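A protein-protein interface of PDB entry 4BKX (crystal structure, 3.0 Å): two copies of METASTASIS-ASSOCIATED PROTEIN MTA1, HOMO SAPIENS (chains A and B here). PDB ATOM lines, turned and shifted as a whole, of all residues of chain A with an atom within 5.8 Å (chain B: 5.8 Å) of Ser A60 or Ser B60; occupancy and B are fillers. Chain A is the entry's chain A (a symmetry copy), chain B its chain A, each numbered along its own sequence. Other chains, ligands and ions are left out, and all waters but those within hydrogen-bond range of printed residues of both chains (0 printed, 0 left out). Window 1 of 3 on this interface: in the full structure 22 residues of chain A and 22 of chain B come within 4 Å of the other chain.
The backbone carbonyl oxygen (O) of Val B56 is in hydrogen-bond range of the side-chain hydroxyl (OG) of Ser B60 (2.9 Å). O of Ser B60 is in hydrogen-bond range of OG1 of Thr B63 (3.2 Å). The side-chain hydroxyl of Ser A60 sits at hydrogen-bond distance from the backbone carbonyl oxygen of Val A56. OG1 of Thr A63 is in hydrogen-bond range of O of Ser A60 (3.2 Å).
Val A57 touches its own counterpart, Val B57. Ser A60 touches Val B61, and with the chains exchanged Val A61 touches Ser B60. Ser A60 touches Phe B64, and with the chains exchanged Phe A64 touches Ser B60. Thr A63 touches Phe B64, and with the chains exchanged Phe A64 touches Thr B63. Positions printed for both chains: 55, 56, 57, 58, 59, 60, 61, 62, 63, 64, 65, 86 and 119.
Ser A60 touches just these residues of chain B: Ser B60 (3.6 Å), Val B61 (3.7 Å) and Phe B64 (3.2 Å). Gly A62 touches none of the printed residues of chain B. Of the printed residues of chain B, Phe A64 touches Val B56 (3.96 Å), Ser B60 (3.2 Å) and Thr B63 (3.5 Å). Printed residues of chain A within 4 Å of Val B57: Val A57. Ser B60 touches just these residues of chain A: Ser A60 (3.6 Å), Val A61 (3.7 Å) and Phe A64 (3.2 Å). Of the printed residues of chain A, Val B61 touches Ser A60. Of the printed residues of chain A, Thr B63 touches Thr A63 (3.0 Å) and Phe A64 (3.5 Å). Printed residues of chain A within 4 Å of Phe B64: Val A56 (3.96 Å), Ser A60 (3.2 Å) and Thr A63 (3.5 Å). The nearest residue of chain B that does not touch Ser A60 is Thr B63 (4.5 Å).
Hydrophobic or aromatic side chains of chain B that line the printed part of chain A: Val B56, Val B57 and Phe B64. Printed residues of chain A that touch a printed residue of chain B: Val A56, Val A57, Ser A60, Val A61, Thr A63 and Phe A64. Among the printed residues, 11 pairs touch across the chains. Among the printed residues, no Asp or Glu carboxylate lies within 4 Å of a Lys or Arg side-chain nitrogen of the other chain.
Among the printed residues, merely in contact across the chains: Val A56 with Phe B64 (3.96 Å), Val A57 with Val B57 (3.5 Å), Ser A60 with Ser B60 (3.6 Å), Ser A60 with Val B61 (3.7 Å), Ser A60 with Phe B64 (3.2 Å), Val A61 with Ser B60 (3.7 Å), Thr A63 with Phe B64 (3.5 Å), Phe A64 with Val B56 (3.96 Å), Phe A64 with Ser B60 (3.2 Å) and Phe A64 with Thr B63 (3.5 Å).
The side-chain hydroxyl of Thr B63 sits at hydrogen-bond distance from the side-chain hydroxyl of Thr A63.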
ATOM      1  N   LEU A  55     -12.803   6.528  20.410  1.00  0.00           N
ATOM      2  CA  LEU A  55     -11.444   6.628  19.869  1.00  0.00           C
ATOM      3  C   LEU A  55     -11.184   7.971  19.186  1.00  0.00           C
ATOM      4  O   LEU A  55     -10.040   8.436  19.135  1.00  0.00           O
ATOM      5  CB  LEU A  55     -11.134   5.476  18.904  1.00  0.00           C
ATOM      6  CG  LEU A  55     -11.084   4.026  19.404  1.00  0.00           C
ATOM      7  CD1 LEU A  55     -10.366   3.149  18.387  1.00  0.00           C
ATOM      8  CD2 LEU A  55     -10.422   3.890  20.767  1.00  0.00           C
ATOM      9  N   VAL A  56     -12.241   8.584  18.655  1.00  0.00           N
ATOM     10  CA  VAL A  56     -12.145   9.932  18.100  1.00  0.00           C
ATOM     11  C   VAL A  56     -11.953  10.917  19.247  1.00  0.00           C
ATOM     12  O   VAL A  56     -11.112  11.818  19.166  1.00  0.00           O
ATOM     13  CB  VAL A  56     -13.392  10.324  17.272  1.00  0.00           C
ATOM     14  CG1 VAL A  56     -13.238  11.720  16.691  1.00  0.00           C
ATOM     15  CG2 VAL A  56     -13.630   9.330  16.148  1.00  0.00           C
ATOM     16  N   VAL A  57     -12.725  10.727  20.316  1.00  0.00           N
ATOM     17  CA  VAL A  57     -12.644  11.587  21.493  1.00  0.00           C
ATOM     18  C   VAL A  57     -11.271  11.468  22.147  1.00  0.00           C
ATOM     19  O   VAL A  57     -10.679  12.473  22.538  1.00  0.00           O
ATOM     20  CB  VAL A  57     -13.751  11.268  22.520  1.00  0.00           C
ATOM     21  CG1 VAL A  57     -13.667  12.215  23.714  1.00  0.00           C
ATOM     22  CG2 VAL A  57     -15.123  11.377  21.877  1.00  0.00           C
ATOM     23  N   ALA A  58     -10.766  10.240  22.244  1.00  0.00           N
ATOM     24  CA  ALA A  58      -9.446   9.976  22.820  1.00  0.00           C
ATOM     25  C   ALA A  58      -8.351  10.669  22.022  1.00  0.00           C
ATOM     26  O   ALA A  58      -7.399  11.202  22.593  1.00  0.00           O
ATOM     27  CB  ALA A  58      -9.185   8.483  22.890  1.00  0.00           C
ATOM     28  N   ARG A  59      -8.500  10.653  20.701  1.00  0.00           N
ATOM     29  CA  ARG A  59      -7.591  11.345  19.803  1.00  0.00           C
ATOM     30  C   ARG A  59      -7.699  12.852  19.947  1.00  0.00           C
ATOM     31  O   ARG A  59      -6.688  13.551  19.886  1.00  0.00           O
ATOM     32  CB  ARG A  59      -7.885  10.959  18.361  1.00  0.00           C
ATOM     33  CG  ARG A  59      -7.033   9.825  17.842  1.00  0.00           C
ATOM     34  CD  ARG A  59      -7.314   9.612  16.374  1.00  0.00           C
ATOM     35  NE  ARG A  59      -8.261   8.530  16.175  1.00  0.00           N
ATOM     36  CZ  ARG A  59      -8.994   8.372  15.081  1.00  0.00           C
ATOM     37  NH1 ARG A  59      -8.898   9.252  14.084  1.00  0.00           N
ATOM     38  NH2 ARG A  59      -9.831   7.340  14.992  1.00  0.00           N
ATOM     39  N   SER A  60      -8.929  13.338  20.128  1.00  0.00           N
ATOM     40  CA  SER A  60      -9.197  14.763  20.286  1.00  0.00           C
ATOM     41  C   SER A  60      -8.544  15.304  21.544  1.00  0.00           C
ATOM     42  O   SER A  60      -7.847  16.317  21.501  1.00  0.00           O
ATOM     43  CB  SER A  60     -10.697  15.024  20.324  1.00  0.00           C
ATOM     44  OG  SER A  60     -11.293  14.729  19.079  1.00  0.00           O
ATOM     45  N   VAL A  61      -8.770  14.612  22.659  1.00  0.00           N
ATOM     46  CA  VAL A  61      -8.132  14.946  23.931  1.00  0.00           C
ATOM     47  C   VAL A  61      -6.606  14.960  23.783  1.00  0.00           C
ATOM     48  O   VAL A  61      -5.928  15.830  24.334  1.00  0.00           O
ATOM     49  CB  VAL A  61      -8.573  13.979  25.055  1.00  0.00           C
ATOM     50  CG1 VAL A  61      -7.851  14.282  26.357  1.00  0.00           C
ATOM     51  CG2 VAL A  61     -10.077  14.069  25.269  1.00  0.00           C
ATOM     52  N   GLY A  62      -6.085  14.010  23.012  1.00  0.00           N
ATOM     53  CA  GLY A  62      -4.659  13.926  22.727  1.00  0.00           C
ATOM     54  C   GLY A  62      -4.103  15.168  22.062  1.00  0.00           C
ATOM     55  O   GLY A  62      -3.077  15.689  22.498  1.00  0.00           O
ATOM     56  N   THR A  63      -4.777  15.644  21.010  1.00  0.00           N
ATOM     57  CA  THR A  63      -4.308  16.825  20.269  1.00  0.00           C
ATOM     58  C   THR A  63      -4.413  18.076  21.135  1.00  0.00           C
ATOM     59  O   THR A  63      -3.512  18.914  21.138  1.00  0.00           O
ATOM     60  CB  THR A  63      -5.058  17.067  18.933  1.00  0.00           C
ATOM     61  OG1 THR A  63      -6.250  17.819  19.173  1.00  0.00           O
ATOM     62  CG2 THR A  63      -5.421  15.775  18.247  1.00  0.00           C
ATOM     63  N   PHE A  64      -5.513  18.191  21.873  1.00  0.00           N
ATOM     64  CA  PHE A  64      -5.714  19.326  22.760  1.00  0.00           C
ATOM     65  C   PHE A  64      -4.663  19.347  23.858  1.00  0.00           C
ATOM     66  O   PHE A  64      -4.184  20.413  24.232  1.00  0.00           O
ATOM     67  CB  PHE A  64      -7.119  19.313  23.368  1.00  0.00           C
ATOM     68  CG  PHE A  64      -7.446  20.543  24.175  1.00  0.00           C
ATOM     69  CD1 PHE A  64      -7.705  21.756  23.549  1.00  0.00           C
ATOM     70  CD2 PHE A  64      -7.496  20.487  25.561  1.00  0.00           C
ATOM     71  CE1 PHE A  64      -8.006  22.890  24.288  1.00  0.00           C
ATOM     72  CE2 PHE A  64      -7.798  21.615  26.306  1.00  0.00           C
ATOM     73  CZ  PHE A  64      -8.053  22.819  25.669  1.00  0.00           C
ATOM     74  N   ALA A  65      -4.313  18.167  24.368  1.00  0.00           N
ATOM     75  CA  ALA A  65      -3.291  18.049  25.399  1.00  0.00           C
ATOM     76  C   ALA A  65      -1.980  18.638  24.913  1.00  0.00           C
ATOM     77  O   ALA A  65      -1.409  19.518  25.560  1.00  0.00           O
ATOM     78  CB  ALA A  65      -3.099  16.599  25.804  1.00  0.00           C
ATOM     79  N   ALA A  86      -1.349  12.467  17.926  1.00  0.00           N
ATOM     80  CA  ALA A  86      -2.379  11.938  18.818  1.00  0.00           C
ATOM     81  C   ALA A  86      -3.157  10.767  18.206  1.00  0.00           C
ATOM     82  O   ALA A  86      -3.841  10.034  18.918  1.00  0.00           O
ATOM     83  CB  ALA A  86      -3.327  13.047  19.241  1.00  0.00           C
ATOM     84  N   PRO A 119      -6.013  17.280  30.315  1.00  0.00           N
ATOM     85  CA  PRO A 119      -5.966  16.130  29.414  1.00  0.00           C
ATOM     86  C   PRO A 119      -4.777  15.213  29.696  1.00  0.00           C
ATOM     87  O   PRO A 119      -3.931  15.539  30.527  1.00  0.00           O
ATOM     88  CB  PRO A 119      -5.824  16.773  28.024  1.00  0.00           C
ATOM     89  CG  PRO A 119      -5.876  18.257  28.226  1.00  0.00           C
ATOM     90  CD  PRO A 119      -5.519  18.501  29.657  1.00  0.00           C
ATOM     91  N   LEU B  55     -16.493  20.192  29.301  1.00  0.00           N
ATOM     92  CA  LEU B  55     -16.124  21.397  28.553  1.00  0.00           C
ATOM     93  C   LEU B  55     -14.707  21.322  27.983  1.00  0.00           C
ATOM     94  O   LEU B  55     -14.410  21.946  26.958  1.00  0.00           O
ATOM     95  CB  LEU B  55     -16.283  22.663  29.405  1.00  0.00           C
ATOM     96  CG  LEU B  55     -17.667  23.105  29.901  1.00  0.00           C
ATOM     97  CD1 LEU B  55     -17.621  24.560  30.347  1.00  0.00           C
ATOM     98  CD2 LEU B  55     -18.760  22.914  28.861  1.00  0.00           C
ATOM     99  N   VAL B  56     -13.835  20.569  28.652  1.00  0.00           N
ATOM    100  CA  VAL B  56     -12.493  20.307  28.134  1.00  0.00           C
ATOM    101  C   VAL B  56     -12.611  19.378  26.931  1.00  0.00           C
ATOM    102  O   VAL B  56     -11.966  19.601  25.903  1.00  0.00           O
ATOM    103  CB  VAL B  56     -11.559  19.679  29.196  1.00  0.00           C
ATOM    104  CG1 VAL B  56     -10.170  19.450  28.623  1.00  0.00           C
ATOM    105  CG2 VAL B  56     -11.462  20.567  30.425  1.00  0.00           C
ATOM    106  N   VAL B  57     -13.448  18.351  27.064  1.00  0.00           N
ATOM    107  CA  VAL B  57     -13.669  17.387  25.991  1.00  0.00           C
ATOM    108  C   VAL B  57     -14.296  18.070  24.780  1.00  0.00           C
ATOM    109  O   VAL B  57     -13.893  17.817  23.645  1.00  0.00           O
ATOM    110  CB  VAL B  57     -14.549  16.203  26.448  1.00  0.00           C
ATOM    111  CG1 VAL B  57     -14.719  15.192  25.318  1.00  0.00           C
ATOM    112  CG2 VAL B  57     -13.936  15.520  27.658  1.00  0.00           C
ATOM    113  N   ALA B  58     -15.266  18.946  25.031  1.00  0.00           N
ATOM    114  CA  ALA B  58     -15.938  19.700  23.970  1.00  0.00           C
ATOM    115  C   ALA B  58     -14.953  20.580  23.215  1.00  0.00           C
ATOM    116  O   ALA B  58     -15.032  20.706  21.992  1.00  0.00           O
ATOM    117  CB  ALA B  58     -17.064  20.540  24.546  1.00  0.00           C
ATOM    118  N   ARG B  59     -14.028  21.182  23.956  1.00  0.00           N
ATOM    119  CA  ARG B  59     -12.963  21.982  23.380  1.00  0.00           C
ATOM    120  C   ARG B  59     -11.987  21.132  22.587  1.00  0.00           C
ATOM    121  O   ARG B  59     -11.508  21.559  21.536  1.00  0.00           O
ATOM    122  CB  ARG B  59     -12.207  22.718  24.476  1.00  0.00           C
ATOM    123  CG  ARG B  59     -12.700  24.123  24.728  1.00  0.00           C
ATOM    124  CD  ARG B  59     -11.804  24.801  25.736  1.00  0.00           C
ATOM    125  NE  ARG B  59     -12.376  24.735  27.070  1.00  0.00           N
ATOM    126  CZ  ARG B  59     -11.675  24.868  28.189  1.00  0.00           C
ATOM    127  NH1 ARG B  59     -10.357  25.057  28.129  1.00  0.00           N
ATOM    128  NH2 ARG B  59     -12.296  24.799  29.365  1.00  0.00           N
ATOM    129  N   SER B  60     -11.694  19.938  23.106  1.00  0.00           N
ATOM    130  CA  SER B  60     -10.777  19.004  22.463  1.00  0.00           C
ATOM    131  C   SER B  60     -11.315  18.550  21.120  1.00  0.00           C
ATOM    132  O   SER B  60     -10.608  18.598  20.114  1.00  0.00           O
ATOM    133  CB  SER B  60     -10.527  17.796  23.359  1.00  0.00           C
ATOM    134  OG  SER B  60      -9.826  18.172  24.526  1.00  0.00           O
ATOM    135  N   VAL B  61     -12.574  18.118  21.114  1.00  0.00           N
ATOM    136  CA  VAL B  61     -13.269  17.741  19.885  1.00  0.00           C
ATOM    137  C   VAL B  61     -13.247  18.897  18.877  1.00  0.00           C
ATOM    138  O   VAL B  61     -13.057  18.684  17.677  1.00  0.00           O
ATOM    139  CB  VAL B  61     -14.716  17.281  20.171  1.00  0.00           C
ATOM    140  CG1 VAL B  61     -15.459  16.963  18.884  1.00  0.00           C
ATOM    141  CG2 VAL B  61     -14.712  16.057  21.076  1.00  0.00           C
ATOM    142  N   GLY B  62     -13.413  20.117  19.381  1.00  0.00           N
ATOM    143  CA  GLY B  62     -13.360  21.319  18.563  1.00  0.00           C
ATOM    144  C   GLY B  62     -12.045  21.491  17.830  1.00  0.00           C
ATOM    145  O   GLY B  62     -12.043  21.747  16.626  1.00  0.00           O
ATOM    146  N   THR B  63     -10.928  21.350  18.551  1.00  0.00           N
ATOM    147  CA  THR B  63      -9.598  21.529  17.948  1.00  0.00           C
ATOM    148  C   THR B  63      -9.310  20.415  16.946  1.00  0.00           C
ATOM    149  O   THR B  63      -8.773  20.666  15.868  1.00  0.00           O
ATOM    150  CB  THR B  63      -8.443  21.592  18.982  1.00  0.00           C
ATOM    151  OG1 THR B  63      -8.005  20.270  19.305  1.00  0.00           O
ATOM    152  CG2 THR B  63      -8.857  22.298  20.249  1.00  0.00           C
ATOM    153  N   PHE B  64      -9.680  19.190  17.306  1.00  0.00           N
ATOM    154  CA  PHE B  64      -9.484  18.051  16.422  1.00  0.00           C
ATOM    155  C   PHE B  64     -10.303  18.205  15.151  1.00  0.00           C
ATOM    156  O   PHE B  64      -9.838  17.853  14.072  1.00  0.00           O
ATOM    157  CB  PHE B  64      -9.834  16.737  17.125  1.00  0.00           C
ATOM    158  CG  PHE B  64      -9.508  15.507  16.318  1.00  0.00           C
ATOM    159  CD1 PHE B  64      -8.191  15.094  16.154  1.00  0.00           C
ATOM    160  CD2 PHE B  64     -10.516  14.762  15.723  1.00  0.00           C
ATOM    161  CE1 PHE B  64      -7.886  13.962  15.413  1.00  0.00           C
ATOM    162  CE2 PHE B  64     -10.219  13.631  14.982  1.00  0.00           C
ATOM    163  CZ  PHE B  64      -8.902  13.230  14.826  1.00  0.00           C
ATOM    164  N   ALA B  65     -11.520  18.730  15.289  1.00  0.00           N
ATOM    165  CA  ALA B  65     -12.389  18.963  14.144  1.00  0.00           C
ATOM    166  C   ALA B  65     -11.709  19.879  13.143  1.00  0.00           C
ATOM    167  O   ALA B  65     -11.573  19.533  11.968  1.00  0.00           O
ATOM    168  CB  ALA B  65     -13.715  19.556  14.585  1.00  0.00           C
ATOM    169  N   ALA B  86     -11.228  26.891  19.299  1.00  0.00           N
ATOM    170  CA  ALA B  86     -12.166  25.931  19.878  1.00  0.00           C
ATOM    171  C   ALA B  86     -12.522  26.246  21.335  1.00  0.00           C
ATOM    172  O   ALA B  86     -13.501  25.722  21.866  1.00  0.00           O
ATOM    173  CB  ALA B  86     -11.619  24.520  19.754  1.00  0.00           C
ATOM    174  N   PRO B 119     -16.218  14.780  14.120  1.00  0.00           N
ATOM    175  CA  PRO B 119     -16.405  15.824  15.126  1.00  0.00           C
ATOM    176  C   PRO B 119     -17.328  16.943  14.644  1.00  0.00           C
ATOM    177  O   PRO B 119     -17.730  16.952  13.483  1.00  0.00           O
ATOM    178  CB  PRO B 119     -14.982  16.363  15.347  1.00  0.00           C
ATOM    179  CG  PRO B 119     -14.068  15.532  14.501  1.00  0.00           C
ATOM    180  CD  PRO B 119     -14.920  14.914  13.440  1.00  0.00           C
